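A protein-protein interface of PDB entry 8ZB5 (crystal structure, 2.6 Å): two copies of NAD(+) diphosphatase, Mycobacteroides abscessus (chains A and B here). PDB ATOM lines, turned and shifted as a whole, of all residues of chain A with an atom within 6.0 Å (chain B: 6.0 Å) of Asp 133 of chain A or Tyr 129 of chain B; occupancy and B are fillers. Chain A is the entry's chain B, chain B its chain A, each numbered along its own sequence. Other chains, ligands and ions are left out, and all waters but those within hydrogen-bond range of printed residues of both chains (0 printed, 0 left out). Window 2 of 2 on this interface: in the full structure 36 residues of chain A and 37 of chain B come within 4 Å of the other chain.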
ATOM      1  N   TYR A 129      -6.555  -6.666  25.079  1.00  0.00           N
ATOM      2  CA  TYR A 129      -7.028  -5.888  26.215  1.00  0.00           C
ATOM      3  C   TYR A 129      -8.514  -6.174  26.448  1.00  0.00           C
ATOM      4  O   TYR A 129      -9.274  -6.344  25.500  1.00  0.00           O
ATOM      5  CB  TYR A 129      -6.697  -4.408  25.985  1.00  0.00           C
ATOM      6  CG  TYR A 129      -5.213  -4.161  25.737  1.00  0.00           C
ATOM      7  CD1 TYR A 129      -4.304  -4.107  26.788  1.00  0.00           C
ATOM      8  CD2 TYR A 129      -4.711  -4.031  24.448  1.00  0.00           C
ATOM      9  CE1 TYR A 129      -2.948  -3.917  26.568  1.00  0.00           C
ATOM     10  CE2 TYR A 129      -3.358  -3.835  24.214  1.00  0.00           C
ATOM     11  CZ  TYR A 129      -2.475  -3.773  25.278  1.00  0.00           C
ATOM     12  OH  TYR A 129      -1.144  -3.572  25.055  1.00  0.00           O
ATOM     13  N   SER A 130      -8.909  -6.274  27.725  1.00  0.00           N
ATOM     14  CA  SER A 130     -10.306  -6.403  28.091  1.00  0.00           C
ATOM     15  C   SER A 130     -11.068  -5.150  27.670  1.00  0.00           C
ATOM     16  O   SER A 130     -10.666  -4.032  27.980  1.00  0.00           O
ATOM     17  CB  SER A 130     -10.502  -6.653  29.562  1.00  0.00           C
ATOM     18  OG  SER A 130     -11.851  -6.387  29.941  1.00  0.00           O
ATOM     19  N   PRO A 131     -12.220  -5.308  26.981  1.00  0.00           N
ATOM     20  CA  PRO A 131     -13.100  -4.179  26.682  1.00  0.00           C
ATOM     21  C   PRO A 131     -13.775  -3.618  27.927  1.00  0.00           C
ATOM     22  O   PRO A 131     -14.369  -2.531  27.882  1.00  0.00           O
ATOM     23  CB  PRO A 131     -14.148  -4.747  25.688  1.00  0.00           C
ATOM     24  CG  PRO A 131     -13.687  -6.171  25.366  1.00  0.00           C
ATOM     25  CD  PRO A 131     -12.711  -6.587  26.436  1.00  0.00           C
ATOM     26  N   VAL A 132     -13.715  -4.407  29.011  1.00  0.00           N
ATOM     27  CA  VAL A 132     -14.523  -4.176  30.197  1.00  0.00           C
ATOM     28  C   VAL A 132     -13.821  -3.139  31.066  1.00  0.00           C
ATOM     29  O   VAL A 132     -14.410  -2.103  31.369  1.00  0.00           O
ATOM     30  CB  VAL A 132     -14.788  -5.484  30.977  1.00  0.00           C
ATOM     31  CG1 VAL A 132     -15.733  -5.265  32.159  1.00  0.00           C
ATOM     32  CG2 VAL A 132     -15.308  -6.597  30.066  1.00  0.00           C
ATOM     33  N   ASP A 133     -12.554  -3.421  31.408  1.00  0.00           N
ATOM     34  CA  ASP A 133     -11.757  -2.569  32.285  1.00  0.00           C
ATOM     35  C   ASP A 133     -10.598  -1.890  31.536  1.00  0.00           C
ATOM     36  O   ASP A 133     -10.306  -0.723  31.790  1.00  0.00           O
ATOM     37  CB  ASP A 133     -11.304  -3.353  33.512  1.00  0.00           C
ATOM     38  CG  ASP A 133     -10.464  -4.587  33.219  1.00  0.00           C
ATOM     39  OD1 ASP A 133      -9.842  -4.623  32.144  1.00  0.00           O
ATOM     40  OD2 ASP A 133     -10.462  -5.516  34.048  1.00  0.00           O
ATOM     41  N   GLY A 134      -9.917  -2.618  30.642  1.00  0.00           N
ATOM     42  CA  GLY A 134      -8.745  -2.104  29.951  1.00  0.00           C
ATOM     43  C   GLY A 134      -7.509  -2.987  30.152  1.00  0.00           C
ATOM     44  O   GLY A 134      -6.475  -2.747  29.540  1.00  0.00           O
ATOM     45  N   SER A 135      -7.607  -4.024  30.985  1.00  0.00           N
ATOM     46  CA  SER A 135      -6.429  -4.770  31.401  1.00  0.00           C
ATOM     47  C   SER A 135      -5.833  -5.531  30.224  1.00  0.00           C
ATOM     48  O   SER A 135      -6.559  -5.978  29.364  1.00  0.00           O
ATOM     49  CB  SER A 135      -6.746  -5.727  32.530  1.00  0.00           C
ATOM     50  OG  SER A 135      -7.258  -5.027  33.653  1.00  0.00           O
ATOM     51  N   PRO A 136      -4.498  -5.739  30.162  1.00  0.00           N
ATOM     52  CA  PRO A 136      -3.918  -6.761  29.284  1.00  0.00           C
ATOM     53  C   PRO A 136      -4.697  -8.066  29.379  1.00  0.00           C
ATOM     54  O   PRO A 136      -5.392  -8.267  30.364  1.00  0.00           O
ATOM     55  CB  PRO A 136      -2.485  -6.903  29.822  1.00  0.00           C
ATOM     56  CG  PRO A 136      -2.166  -5.506  30.318  1.00  0.00           C
ATOM     57  CD  PRO A 136      -3.476  -4.975  30.898  1.00  0.00           C
ATOM     58  N   ASN A 148      -8.218 -12.243  31.167  1.00  0.00           N
ATOM     59  CA  ASN A 148      -7.889 -10.952  31.741  1.00  0.00           C
ATOM     60  C   ASN A 148      -6.837 -11.170  32.834  1.00  0.00           C
ATOM     61  O   ASN A 148      -6.918 -12.122  33.604  1.00  0.00           O
ATOM     62  CB  ASN A 148      -9.155 -10.249  32.203  1.00  0.00           C
ATOM     63  CG  ASN A 148      -8.861  -8.934  32.880  1.00  0.00           C
ATOM     64  OD1 ASN A 148      -7.840  -8.830  33.566  1.00  0.00           O
ATOM     65  ND2 ASN A 148      -9.713  -7.928  32.708  1.00  0.00           N
ATOM     66  N   ALA A 150      -5.802  -8.974  35.292  1.00  0.00           N
ATOM     67  CA  ALA A 150      -6.254  -8.481  36.580  1.00  0.00           C
ATOM     68  C   ALA A 150      -7.328  -9.397  37.194  1.00  0.00           C
ATOM     69  O   ALA A 150      -7.138  -9.888  38.310  1.00  0.00           O
ATOM     70  CB  ALA A 150      -6.738  -7.056  36.412  1.00  0.00           C
ATOM     71  N   THR A 151      -8.430  -9.654  36.454  1.00  0.00           N
ATOM     72  CA  THR A 151      -9.644 -10.262  36.998  1.00  0.00           C
ATOM     73  C   THR A 151      -9.726 -11.770  36.746  1.00  0.00           C
ATOM     74  O   THR A 151     -10.471 -12.454  37.448  1.00  0.00           O
ATOM     75  CB  THR A 151     -10.912  -9.596  36.448  1.00  0.00           C
ATOM     76  OG1 THR A 151     -11.099 -10.027  35.101  1.00  0.00           O
ATOM     77  CG2 THR A 151     -10.924  -8.082  36.580  1.00  0.00           C
ATOM     78  N   ASN B 126     -19.652  -3.031  29.076  1.00  0.00           N
ATOM     79  CA  ASN B 126     -18.560  -3.969  28.846  1.00  0.00           C
ATOM     80  C   ASN B 126     -17.674  -3.556  27.663  1.00  0.00           C
ATOM     81  O   ASN B 126     -16.999  -4.403  27.085  1.00  0.00           O
ATOM     82  CB  ASN B 126     -19.058  -5.383  28.559  1.00  0.00           C
ATOM     83  CG  ASN B 126     -19.697  -6.045  29.751  1.00  0.00           C
ATOM     84  OD1 ASN B 126     -19.112  -6.966  30.327  1.00  0.00           O
ATOM     85  ND2 ASN B 126     -20.906  -5.631  30.099  1.00  0.00           N
ATOM     86  N   ALA B 127     -17.651  -2.269  27.302  1.00  0.00           N
ATOM     87  CA  ALA B 127     -16.879  -1.831  26.148  1.00  0.00           C
ATOM     88  C   ALA B 127     -16.406  -0.393  26.348  1.00  0.00           C
ATOM     89  O   ALA B 127     -16.505   0.439  25.452  1.00  0.00           O
ATOM     90  CB  ALA B 127     -17.707  -1.984  24.886  1.00  0.00           C
ATOM     91  N   GLY B 128     -15.872  -0.115  27.539  1.00  0.00           N
ATOM     92  CA  GLY B 128     -15.382   1.214  27.862  1.00  0.00           C
ATOM     93  C   GLY B 128     -13.923   1.374  27.444  1.00  0.00           C
ATOM     94  O   GLY B 128     -13.372   2.468  27.547  1.00  0.00           O
ATOM     95  N   TYR B 129     -13.317   0.274  26.971  1.00  0.00           N
ATOM     96  CA  TYR B 129     -11.929   0.256  26.549  1.00  0.00           C
ATOM     97  C   TYR B 129     -11.808  -0.514  25.233  1.00  0.00           C
ATOM     98  O   TYR B 129     -12.498  -1.510  25.027  1.00  0.00           O
ATOM     99  CB  TYR B 129     -11.111  -0.317  27.716  1.00  0.00           C
ATOM    100  CG  TYR B 129     -11.224   0.522  28.986  1.00  0.00           C
ATOM    101  CD1 TYR B 129     -12.310   0.381  29.846  1.00  0.00           C
ATOM    102  CD2 TYR B 129     -10.272   1.484  29.306  1.00  0.00           C
ATOM    103  CE1 TYR B 129     -12.443   1.163  30.984  1.00  0.00           C
ATOM    104  CE2 TYR B 129     -10.392   2.268  30.444  1.00  0.00           C
ATOM    105  CZ  TYR B 129     -11.478   2.105  31.287  1.00  0.00           C
ATOM    106  OH  TYR B 129     -11.608   2.863  32.410  1.00  0.00           O
ATOM    107  N   SER B 130     -10.935  -0.027  24.340  1.00  0.00           N
ATOM    108  CA  SER B 130     -10.627  -0.736  23.111  1.00  0.00           C
ATOM    109  C   SER B 130      -9.978  -2.084  23.423  1.00  0.00           C
ATOM    110  O   SER B 130      -9.022  -2.161  24.184  1.00  0.00           O
ATOM    111  CB  SER B 130      -9.739   0.068  22.186  1.00  0.00           C
ATOM    112  OG  SER B 130      -9.146  -0.769  21.193  1.00  0.00           O
ATOM    113  N   PRO B 131     -10.458  -3.182  22.805  1.00  0.00           N
ATOM    114  CA  PRO B 131      -9.799  -4.483  22.908  1.00  0.00           C
ATOM    115  C   PRO B 131      -8.459  -4.516  22.186  1.00  0.00           C
ATOM    116  O   PRO B 131      -7.700  -5.487  22.338  1.00  0.00           O
ATOM    117  CB  PRO B 131     -10.784  -5.487  22.250  1.00  0.00           C
ATOM    118  CG  PRO B 131     -12.020  -4.694  21.903  1.00  0.00           C
ATOM    119  CD  PRO B 131     -11.677  -3.226  21.985  1.00  0.00           C
ATOM    120  N   VAL B 132      -8.235  -3.489  21.348  1.00  0.00           N
ATOM    121  CA  VAL B 132      -7.118  -3.486  20.420  1.00  0.00           C
ATOM    122  C   VAL B 132      -5.878  -3.002  21.164  1.00  0.00           C
ATOM    123  O   VAL B 132      -4.889  -3.728  21.232  1.00  0.00           O
ATOM    124  CB  VAL B 132      -7.389  -2.638  19.159  1.00  0.00           C
ATOM    125  CG1 VAL B 132      -6.272  -2.794  18.130  1.00  0.00           C
ATOM    126  CG2 VAL B 132      -8.734  -2.980  18.523  1.00  0.00           C
ATOM    127  N   GLY B 134      -6.271  -0.705  24.361  1.00  0.00           N
ATOM    128  CA  GLY B 134      -6.550  -0.516  25.778  1.00  0.00           C
ATOM    129  C   GLY B 134      -7.146   0.861  26.081  1.00  0.00           C
ATOM    130  O   GLY B 134      -7.522   1.145  27.210  1.00  0.00           O
ATOM    131  N   SER B 135      -7.232   1.740  25.083  1.00  0.00           N
ATOM    132  CA  SER B 135      -7.601   3.126  25.326  1.00  0.00           C
ATOM    133  C   SER B 135      -9.036   3.226  25.839  1.00  0.00           C
ATOM    134  O   SER B 135      -9.879   2.423  25.461  1.00  0.00           O
ATOM    135  CB  SER B 135      -7.431   3.954  24.074  1.00  0.00           C
ATOM    136  OG  SER B 135      -6.093   3.887  23.595  1.00  0.00           O
ATOM    137  N   PRO B 136      -9.376   4.220  26.691  1.00  0.00           N
ATOM    138  CA  PRO B 136     -10.779   4.564  26.942  1.00  0.00           C
ATOM    139  C   PRO B 136     -11.540   4.631  25.624  1.00  0.00           C
ATOM    140  O   PRO B 136     -10.913   4.815  24.591  1.00  0.00           O
ATOM    141  CB  PRO B 136     -10.730   5.943  27.651  1.00  0.00           C
ATOM    142  CG  PRO B 136      -9.324   6.032  28.239  1.00  0.00           C
ATOM    143  CD  PRO B 136      -8.440   5.024  27.495  1.00  0.00           C
ATOM    144  N   THR B 137     -12.876   4.498  25.676  1.00  0.00           N
ATOM    145  CA  THR B 137     -13.731   4.664  24.508  1.00  0.00           C
ATOM    146  C   THR B 137     -14.881   5.571  24.919  1.00  0.00           C
ATOM    147  O   THR B 137     -15.178   5.652  26.101  1.00  0.00           O
ATOM    148  CB  THR B 137     -14.250   3.326  23.979  1.00  0.00           C
ATOM    149  OG1 THR B 137     -15.176   2.812  24.925  1.00  0.00           O
ATOM    150  CG2 THR B 137     -13.179   2.270  23.776  1.00  0.00           C
ATOM    151  N   ARG B 146     -18.901   3.180  20.115  1.00  0.00           N
ATOM    152  CA  ARG B 146     -17.954   3.805  21.008  1.00  0.00           C
ATOM    153  C   ARG B 146     -16.668   4.084  20.237  1.00  0.00           C
ATOM    154  O   ARG B 146     -16.069   3.181  19.649  1.00  0.00           O
ATOM    155  CB  ARG B 146     -17.719   2.908  22.224  1.00  0.00           C
ATOM    156  CG  ARG B 146     -18.939   2.823  23.129  1.00  0.00           C
ATOM    157  CD  ARG B 146     -18.670   1.950  24.338  1.00  0.00           C
ATOM    158  NE  ARG B 146     -17.960   2.648  25.415  1.00  0.00           N
ATOM    159  CZ  ARG B 146     -18.503   3.517  26.272  1.00  0.00           C
ATOM    160  NH1 ARG B 146     -19.791   3.815  26.238  1.00  0.00           N
ATOM    161  NH2 ARG B 146     -17.743   4.089  27.184  1.00  0.00           N
ATOM    162  N   GLU B 155     -15.746   1.217  17.733  1.00  0.00           N
ATOM    163  CA  GLU B 155     -16.086  -0.105  18.237  1.00  0.00           C
ATOM    164  C   GLU B 155     -17.603  -0.264  18.154  1.00  0.00           C
ATOM    165  O   GLU B 155     -18.329   0.718  18.328  1.00  0.00           O
ATOM    166  CB  GLU B 155     -15.543  -0.291  19.656  1.00  0.00           C
ATOM    167  CG  GLU B 155     -14.023  -0.396  19.724  1.00  0.00           C
ATOM    168  CD  GLU B 155     -13.463  -1.690  19.163  1.00  0.00           C
ATOM    169  OE1 GLU B 155     -12.401  -1.622  18.514  1.00  0.00           O
ATOM    170  OE2 GLU B 155     -14.074  -2.769  19.351  1.00  0.00           O
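O of Pro 131 of chain A lies within hydrogen-bond range of N of Tyr 129 of chain B.
The backbone carbonyl oxygen (O) of Pro 131 of chain B lies within hydrogen-bond range of the backbone NH (N) of Tyr 129 of chain A, at 3.2 Å.
O of Pro 131 of chain A is in hydrogen-bond range of N of Gly 128 of chain B (2.9 Å).
O of Pro 131 of chain A sits close to N of Ala 127 of chain B (3.3 Å).
The backbone carbonyl oxygen of Asn 126 of chain B sits close to the backbone carbonyl oxygen of Pro 131 of chain A (3.3 Å).
N of Ser 130 of chain A sits at hydrogen-bond distance from O of Ser 135 of chain A.
The backbone carbonyl oxygen (O) of Gly 128 of chain B sits at hydrogen-bond distance from the backbone NH (N) of Thr 137 of chain B, at 2.8 Å.
N of Ser 135 of chain A is in hydrogen-bond range of OD1 of Asp 133 of chain A, at 2.6 Å.
OD2 of Asp 133 of chain A sits at hydrogen-bond distance from ND2 of Asn 148 of chain A (2.9 Å).
The side-chain hydroxyl (OG) of Ser 130 of chain A sits at hydrogen-bond distance from the backbone NH (N) of Asp 133 of chain A (3.4 Å).
The side-chain hydroxyl (OG1) of Thr 137 of chain B sits at hydrogen-bond distance from the backbone carbonyl oxygen (O) of Ala 127 of chain B (2.8 Å).
Ser 130 of chain B touches Tyr 129 of chain A (O to CB, 3.7 Å).
Val 132 of chain B touches Tyr 129 of chain A.
N of Gly 134 of chain B touches CD2 of Tyr 129 of chain A, at 3.7 Å.
O of Ser 130 of chain A touches CB of Tyr 129 of chain B, at 3.8 Å.
N of Val 132 of chain A touches O of Asn 126 of chain B, 3.8 Å away.
O of Val 132 of chain A touches CD1 of Tyr 129 of chain B, at 3.6 Å.
Tyr 129 of chain B touches Asp 133 of chain A.
CB of Tyr 129 of chain B touches CA of Gly 134 of chain A, 3.7 Å away.
Asp 133 of chain A touches one residue of chain B.
Thr 151 of chain A touches none of the printed residues of chain B.
Of the printed residues of chain A, Asn 126 of chain B touches Pro 131 and Val 132.
Of the printed residues of chain A, Ser 130 of chain B touches Tyr 129 (3.7 Å).
Arg 146 of chain B touches none of the printed residues of chain A.
The nearest residue of chain B that does not touch Asp 133 of chain A is Gly 134 of chain B (5.7 Å).
The nearest printed residue of chain B that does not touch Tyr 129 of chain A is Tyr 129 of chain B (5.8 Å).
Of the 13 printed residues of chain B, 8 touch a printed residue of chain A.
Hydrophobic or aromatic side chains of chain B that line the printed part of chain A: Tyr 129 and Pro 131.
Printed residues of chain A that touch a printed residue of chain B: Tyr 129, Ser 130, Pro 131, Val 132, Asp 133 and Gly 134.
Hydrophobic or aromatic side chains of chain A within 4 Å of the printed part of chain B: Tyr 129, Pro 131 and Val 132.
Along chain A the printed residues that touch a printed residue of chain B span positions 129 to 134.
Among the printed residues, 13 pairs touch across the chains.
Among the printed residues, no Asp or Glu carboxylate lies within 4 Å of a Lys or Arg side-chain nitrogen of the other chain.
Tyr 129 of chain A touches Ser 130 of chain B, and with the chains exchanged Ser 130 of chain A touches Tyr 129 of chain B.
Tyr 129 of chain A touches Pro 131 of chain B, and with the chains exchanged Pro 131 of chain A touches Tyr 129 of chain B.
Tyr 129 of chain A touches Val 132 of chain B, and with the chains exchanged Val 132 of chain A touches Tyr 129 of chain B.
Tyr 129 of chain A touches Gly 134 of chain B, and with the chains exchanged Gly 134 of chain A touches Tyr 129 of chain B.
7 positions are printed for both chains.
Of the 13 pairs that touch across the chains among the printed residues, 8 have their exchanged pair printed and touching as well.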
